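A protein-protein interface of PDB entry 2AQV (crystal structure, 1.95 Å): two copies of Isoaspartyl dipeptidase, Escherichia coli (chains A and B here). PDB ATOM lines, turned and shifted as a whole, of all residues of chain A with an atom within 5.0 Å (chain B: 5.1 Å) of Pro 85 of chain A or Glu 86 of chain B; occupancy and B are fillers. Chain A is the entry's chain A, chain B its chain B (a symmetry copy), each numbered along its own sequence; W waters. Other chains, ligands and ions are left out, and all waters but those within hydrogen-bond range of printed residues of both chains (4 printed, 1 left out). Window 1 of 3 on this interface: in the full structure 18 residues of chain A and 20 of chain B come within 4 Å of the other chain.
Pro 85 of chain A touches Glu 86 of chain B, and with the chains exchanged Glu 86 of chain A touches Pro 85 of chain B.
Of the 11 printed residues of chain B, 3 touch a printed residue of chain A. Of the 10 printed residues of chain A, 4 touch a printed residue of chain B. Along chain A the printed residues that touch a printed residue of chain B span positions 83 to 86. Among the printed residues, 5 pairs touch across the chains.
Among the printed residues, pairs that only touch across the chains: Arg 83 of chain A with Phe 387 of chain B, Thr 84 of chain A with Phe 387 of chain B, Pro 85 of chain A with Glu 86 of chain B, Glu 86 of chain A with Pro 85 of chain B and Pro 85 of chain A with Phe 387 of chain B.
Water W2 lies within hydrogen-bond range of the backbone carbonyl oxygen (O) of Thr 84 of chain A (2.6 Å), the guanidinium group (NH1) of Arg 111 of chain A (2.9 Å) and the side-chain carboxylate (OE2) of Glu 86 of chain B (3.1 Å). Water W1 bridges the backbone carbonyl oxygen (O) of Thr 84 of chain B (2.7 Å) and the side-chain carboxylate (OE2) of Glu 86 of chain A (3.0 Å). Water W3 bridges OE2 of Glu 86 of chain B and O of Arg 83 of chain A. Water W4 bridges NH1 of Arg 83 of chain A (2.9 Å) and OE1 of Glu 86 of chain B (3.0 Å).
The guanidinium group of Arg 111 of chain A lies within hydrogen-bond range of the backbone carbonyl oxygen of Thr 84 of chain A (2.7 Å). OE1 of Glu 86 of chain B lies within salt-bridge range of NZ of Lys 119 of chain B (2.8 Å). O of Asn 287 of chain A lies within hydrogen-bond range of OG1 of Thr 84 of chain A. The backbone carbonyl oxygen (O) of Pro 85 of chain B is in hydrogen-bond range of the side-chain amide nitrogen (ND2) of Asn 287 of chain B, at 2.7 Å.
Printed residues of chain B within 4 Å of Thr 84 of chain A: Phe 387. Pro 85 of chain A touches just these residues of chain B: Glu 86 (3.6 Å) and Phe 387 (3.9 Å). Of the printed residues of chain A, Pro 85 of chain B touches Glu 86. Of chain A, only Pro 85 (3.6 Å) comes within 4 Å of Glu 86 of chain B. Asn 287 of chain B touches none of the printed residues of chain A. The nearest residue of chain A that does not touch Glu 86 of chain B is Thr 84 of chain A (4.5 Å).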
ATOM      1  N   HIS A  70     -19.369  -5.455  21.382  1.00  0.00           N
ATOM      2  CA  HIS A  70     -19.582  -4.276  22.216  1.00  0.00           C
ATOM      3  C   HIS A  70     -20.080  -4.719  23.584  1.00  0.00           C
ATOM      4  O   HIS A  70     -21.264  -4.550  23.942  1.00  0.00           O
ATOM      5  CB  HIS A  70     -20.610  -3.354  21.569  1.00  0.00           C
ATOM      6  CG  HIS A  70     -20.003  -2.862  20.298  1.00  0.00           C
ATOM      7  ND1 HIS A  70     -19.265  -1.680  20.251  1.00  0.00           N
ATOM      8  CD2 HIS A  70     -20.011  -3.445  19.066  1.00  0.00           C
ATOM      9  CE1 HIS A  70     -18.823  -1.567  19.006  1.00  0.00           C
ATOM     10  NE2 HIS A  70     -19.288  -2.593  18.281  1.00  0.00           N
ATOM     11  N   ILE A  72     -19.858  -3.730  26.679  1.00  0.00           N
ATOM     12  CA  ILE A  72     -20.591  -2.854  27.606  1.00  0.00           C
ATOM     13  C   ILE A  72     -21.824  -2.180  26.998  1.00  0.00           C
ATOM     14  O   ILE A  72     -22.514  -1.415  27.655  1.00  0.00           O
ATOM     15  CB  ILE A  72     -19.678  -1.806  28.302  1.00  0.00           C
ATOM     16  CG1 ILE A  72     -19.245  -0.644  27.382  1.00  0.00           C
ATOM     17  CG2 ILE A  72     -18.502  -2.428  29.068  1.00  0.00           C
ATOM     18  CD1 ILE A  72     -18.290   0.380  28.040  1.00  0.00           C
ATOM     19  N   GLY A  73     -22.093  -2.415  25.725  1.00  0.00           N
ATOM     20  CA  GLY A  73     -23.213  -1.729  25.088  1.00  0.00           C
ATOM     21  C   GLY A  73     -22.604  -0.779  24.065  1.00  0.00           C
ATOM     22  O   GLY A  73     -21.431  -0.397  24.189  1.00  0.00           O
ATOM     23  N   ARG A  83     -28.596   3.734  23.251  1.00  0.00           N
ATOM     24  CA  ARG A  83     -27.429   3.156  23.870  1.00  0.00           C
ATOM     25  C   ARG A  83     -27.773   1.706  24.216  1.00  0.00           C
ATOM     26  O   ARG A  83     -28.690   1.426  24.984  1.00  0.00           O
ATOM     27  CB  ARG A  83     -27.017   3.982  25.088  1.00  0.00           C
ATOM     28  CG  ARG A  83     -26.620   5.424  24.743  1.00  0.00           C
ATOM     29  CD  ARG A  83     -26.490   6.258  26.008  1.00  0.00           C
ATOM     30  NE  ARG A  83     -25.275   5.931  26.794  1.00  0.00           N
ATOM     31  CZ  ARG A  83     -25.271   5.293  27.980  1.00  0.00           C
ATOM     32  NH1 ARG A  83     -26.373   4.842  28.585  1.00  0.00           N
ATOM     33  NH2 ARG A  83     -24.119   5.066  28.570  1.00  0.00           N
ATOM     34  N   THR A  84     -27.132   0.744  23.591  1.00  0.00           N
ATOM     35  CA  THR A  84     -27.592  -0.590  23.956  1.00  0.00           C
ATOM     36  C   THR A  84     -26.994  -1.006  25.276  1.00  0.00           C
ATOM     37  O   THR A  84     -26.039  -0.445  25.809  1.00  0.00           O
ATOM     38  CB  THR A  84     -27.260  -1.629  22.880  1.00  0.00           C
ATOM     39  OG1 THR A  84     -25.854  -1.633  22.758  1.00  0.00           O
ATOM     40  CG2 THR A  84     -27.827  -1.137  21.554  1.00  0.00           C
ATOM     41  N   PRO A  85     -27.601  -2.036  25.792  1.00  0.00           N
ATOM     42  CA  PRO A  85     -27.235  -2.597  27.079  1.00  0.00           C
ATOM     43  C   PRO A  85     -26.020  -3.534  26.984  1.00  0.00           C
ATOM     44  O   PRO A  85     -25.619  -3.988  25.899  1.00  0.00           O
ATOM     45  CB  PRO A  85     -28.469  -3.387  27.525  1.00  0.00           C
ATOM     46  CG  PRO A  85     -29.412  -3.501  26.322  1.00  0.00           C
ATOM     47  CD  PRO A  85     -28.856  -2.612  25.224  1.00  0.00           C
ATOM     48  N   GLU A  86     -25.420  -3.821  28.127  1.00  0.00           N
ATOM     49  CA  GLU A  86     -24.251  -4.657  28.166  1.00  0.00           C
ATOM     50  C   GLU A  86     -24.570  -6.090  27.800  1.00  0.00           C
ATOM     51  O   GLU A  86     -25.699  -6.547  27.836  1.00  0.00           O
ATOM     52  CB  GLU A  86     -23.636  -4.583  29.560  1.00  0.00           C
ATOM     53  CG  GLU A  86     -24.401  -5.548  30.485  1.00  0.00           C
ATOM     54  CD  GLU A  86     -23.825  -5.467  31.859  1.00  0.00           C
ATOM     55  OE1 GLU A  86     -22.703  -5.825  32.164  1.00  0.00           O
ATOM     56  OE2 GLU A  86     -24.594  -4.837  32.680  1.00  0.00           O
ATOM     57  N   VAL A  87     -23.541  -6.816  27.413  1.00  0.00           N
ATOM     58  CA  VAL A  87     -23.696  -8.208  27.002  1.00  0.00           C
ATOM     59  C   VAL A  87     -23.792  -9.128  28.202  1.00  0.00           C
ATOM     60  O   VAL A  87     -23.123  -8.955  29.229  1.00  0.00           O
ATOM     61  CB  VAL A  87     -22.521  -8.633  26.111  1.00  0.00           C
ATOM     62  CG1 VAL A  87     -22.630 -10.134  25.884  1.00  0.00           C
ATOM     63  CG2 VAL A  87     -22.644  -7.939  24.773  1.00  0.00           C
ATOM     64  N   ARG A 111     -19.278   6.274  26.944  1.00  0.00           N
ATOM     65  CA  ARG A 111     -18.670   4.914  27.033  1.00  0.00           C
ATOM     66  C   ARG A 111     -17.189   5.122  27.288  1.00  0.00           C
ATOM     67  O   ARG A 111     -16.579   5.963  26.629  1.00  0.00           O
ATOM     68  CB  ARG A 111     -18.804   4.070  25.756  1.00  0.00           C
ATOM     69  CG  ARG A 111     -20.249   3.899  25.270  1.00  0.00           C
ATOM     70  CD  ARG A 111     -21.168   3.198  26.289  1.00  0.00           C
ATOM     71  NE  ARG A 111     -22.447   2.821  25.625  1.00  0.00           N
ATOM     72  CZ  ARG A 111     -23.379   2.029  26.166  1.00  0.00           C
ATOM     73  NH1 ARG A 111     -23.200   1.505  27.367  1.00  0.00           N
ATOM     74  NH2 ARG A 111     -24.526   1.755  25.467  1.00  0.00           N
ATOM     75  N   ASN A 287     -24.035  -6.816  19.843  1.00  0.00           N
ATOM     76  CA  ASN A 287     -24.442  -5.778  20.784  1.00  0.00           C
ATOM     77  C   ASN A 287     -24.313  -4.344  20.293  1.00  0.00           C
ATOM     78  O   ASN A 287     -24.472  -3.398  21.070  1.00  0.00           O
ATOM     79  CB  ASN A 287     -23.912  -5.963  22.207  1.00  0.00           C
ATOM     80  CG  ASN A 287     -25.043  -6.215  23.166  1.00  0.00           C
ATOM     81  OD1 ASN A 287     -26.008  -6.917  22.825  1.00  0.00           O
ATOM     82  ND2 ASN A 287     -24.871  -5.633  24.351  1.00  0.00           N
ATOM     83  N   LEU B  71     -29.156   4.444  38.465  1.00  0.00           N
ATOM     84  CA  LEU B  71     -29.696   4.312  37.129  1.00  0.00           C
ATOM     85  C   LEU B  71     -28.824   3.522  36.176  1.00  0.00           C
ATOM     86  O   LEU B  71     -29.354   2.742  35.386  1.00  0.00           O
ATOM     87  CB  LEU B  71     -29.996   5.715  36.514  1.00  0.00           C
ATOM     88  CG  LEU B  71     -31.092   6.550  37.221  1.00  0.00           C
ATOM     89  CD1 LEU B  71     -31.175   7.865  36.482  1.00  0.00           C
ATOM     90  CD2 LEU B  71     -32.477   5.856  37.128  1.00  0.00           C
ATOM     91  N   ILE B  72     -27.509   3.804  36.195  1.00  0.00           N
ATOM     92  CA  ILE B  72     -26.645   3.106  35.261  1.00  0.00           C
ATOM     93  C   ILE B  72     -26.136   1.766  35.805  1.00  0.00           C
ATOM     94  O   ILE B  72     -25.402   1.062  35.121  1.00  0.00           O
ATOM     95  CB  ILE B  72     -25.492   3.929  34.666  1.00  0.00           C
ATOM     96  CG1 ILE B  72     -24.518   4.395  35.747  1.00  0.00           C
ATOM     97  CG2 ILE B  72     -26.002   5.060  33.761  1.00  0.00           C
ATOM     98  CD1 ILE B  72     -23.223   4.977  35.163  1.00  0.00           C
ATOM     99  N   GLY B  73     -26.526   1.428  37.035  1.00  0.00           N
ATOM    100  CA  GLY B  73     -26.021   0.233  37.666  1.00  0.00           C
ATOM    101  C   GLY B  73     -25.057   0.751  38.754  1.00  0.00           C
ATOM    102  O   GLY B  73     -24.650   1.899  38.756  1.00  0.00           O
ATOM    103  N   THR B  84     -23.696  -4.033  39.005  1.00  0.00           N
ATOM    104  CA  THR B  84     -25.083  -4.289  38.597  1.00  0.00           C
ATOM    105  C   THR B  84     -25.459  -3.680  37.230  1.00  0.00           C
ATOM    106  O   THR B  84     -24.796  -2.799  36.724  1.00  0.00           O
ATOM    107  CB  THR B  84     -26.050  -3.928  39.728  1.00  0.00           C
ATOM    108  OG1 THR B  84     -25.907  -2.558  39.932  1.00  0.00           O
ATOM    109  CG2 THR B  84     -25.585  -4.579  41.036  1.00  0.00           C
ATOM    110  N   PRO B  85     -26.501  -4.194  36.578  1.00  0.00           N
ATOM    111  CA  PRO B  85     -26.919  -3.687  35.278  1.00  0.00           C
ATOM    112  C   PRO B  85     -27.728  -2.373  35.396  1.00  0.00           C
ATOM    113  O   PRO B  85     -28.240  -2.026  36.490  1.00  0.00           O
ATOM    114  CB  PRO B  85     -27.806  -4.800  34.688  1.00  0.00           C
ATOM    115  CG  PRO B  85     -28.106  -5.796  35.815  1.00  0.00           C
ATOM    116  CD  PRO B  85     -27.328  -5.346  37.031  1.00  0.00           C
ATOM    117  N   GLU B  86     -27.848  -1.647  34.287  1.00  0.00           N
ATOM    118  CA  GLU B  86     -28.592  -0.406  34.331  1.00  0.00           C
ATOM    119  C   GLU B  86     -30.053  -0.714  34.640  1.00  0.00           C
ATOM    120  O   GLU B  86     -30.548  -1.827  34.483  1.00  0.00           O
ATOM    121  CB  GLU B  86     -28.457   0.348  33.016  1.00  0.00           C
ATOM    122  CG  GLU B  86     -29.151  -0.369  31.864  1.00  0.00           C
ATOM    123  CD  GLU B  86     -28.993   0.356  30.555  1.00  0.00           C
ATOM    124  OE1 GLU B  86     -29.459   1.431  30.325  1.00  0.00           O
ATOM    125  OE2 GLU B  86     -28.381  -0.318  29.636  1.00  0.00           O
ATOM    126  N   VAL B  87     -30.774   0.273  35.091  1.00  0.00           N
ATOM    127  CA  VAL B  87     -32.180   0.106  35.428  1.00  0.00           C
ATOM    128  C   VAL B  87     -33.076   0.171  34.189  1.00  0.00           C
ATOM    129  O   VAL B  87     -32.845   0.990  33.289  1.00  0.00           O
ATOM    130  CB  VAL B  87     -32.620   1.253  36.370  1.00  0.00           C
ATOM    131  CG1 VAL B  87     -34.112   1.117  36.663  1.00  0.00           C
ATOM    132  CG2 VAL B  87     -31.907   1.034  37.680  1.00  0.00           C
ATOM    133  N   ALA B  88     -34.105  -0.691  34.117  1.00  0.00           N
ATOM    134  CA  ALA B  88     -35.051  -0.637  32.999  1.00  0.00           C
ATOM    135  C   ALA B  88     -36.278   0.231  33.359  1.00  0.00           C
ATOM    136  O   ALA B  88     -36.721   0.231  34.503  1.00  0.00           O
ATOM    137  CB  ALA B  88     -35.548  -2.013  32.616  1.00  0.00           C
ATOM    138  N   LYS B 119     -27.991   8.355  30.461  1.00  0.00           N
ATOM    139  CA  LYS B 119     -29.081   7.510  30.907  1.00  0.00           C
ATOM    140  C   LYS B 119     -30.261   8.326  31.429  1.00  0.00           C
ATOM    141  O   LYS B 119     -31.442   8.018  31.246  1.00  0.00           O
ATOM    142  CB  LYS B 119     -28.554   6.526  31.949  1.00  0.00           C
ATOM    143  CG  LYS B 119     -29.638   5.624  32.542  1.00  0.00           C
ATOM    144  CD  LYS B 119     -30.271   4.641  31.542  1.00  0.00           C
ATOM    145  CE  LYS B 119     -31.261   3.683  32.192  1.00  0.00           C
ATOM    146  NZ  LYS B 119     -31.768   2.626  31.287  1.00  0.00           N
ATOM    147  N   ASN B 287     -31.446  -0.574  42.545  1.00  0.00           N
ATOM    148  CA  ASN B 287     -30.489  -1.035  41.538  1.00  0.00           C
ATOM    149  C   ASN B 287     -29.063  -1.072  42.006  1.00  0.00           C
ATOM    150  O   ASN B 287     -28.124  -1.311  41.237  1.00  0.00           O
ATOM    151  CB  ASN B 287     -30.715  -0.281  40.210  1.00  0.00           C
ATOM    152  CG  ASN B 287     -30.151  -0.978  39.011  1.00  0.00           C
ATOM    153  OD1 ASN B 287     -30.509  -2.132  38.783  1.00  0.00           O
ATOM    154  ND2 ASN B 287     -29.221  -0.330  38.296  1.00  0.00           N
ATOM    155  N   PHE B 387     -34.810  -0.995  24.659  1.00  0.00           N
ATOM    156  CA  PHE B 387     -34.205  -2.329  24.535  1.00  0.00           C
ATOM    157  C   PHE B 387     -34.694  -3.328  25.579  1.00  0.00           C
ATOM    158  O   PHE B 387     -34.076  -4.386  25.791  1.00  0.00           O
ATOM    159  CB  PHE B 387     -32.665  -2.266  24.618  1.00  0.00           C
ATOM    160  CG  PHE B 387     -32.114  -1.332  23.601  1.00  0.00           C
ATOM    161  CD1 PHE B 387     -31.531  -0.115  23.958  1.00  0.00           C
ATOM    162  CD2 PHE B 387     -32.193  -1.720  22.268  1.00  0.00           C
ATOM    163  CE1 PHE B 387     -31.021   0.718  22.965  1.00  0.00           C
ATOM    164  CE2 PHE B 387     -31.697  -0.881  21.263  1.00  0.00           C
ATOM    165  CZ  PHE B 387     -31.102   0.324  21.627  1.00  0.00           C
HETATM  166  O   HOH W   1     -23.667  -2.475  34.330  1.00  0.00           O
HETATM  167  O   HOH W   2     -25.746   0.496  28.194  1.00  0.00           O
HETATM  168  O   HOH W   3     -29.816  -0.073  27.248  1.00  0.00           O
HETATM  169  O   HOH W   4     -26.882   2.942  30.774  1.00  0.00           O
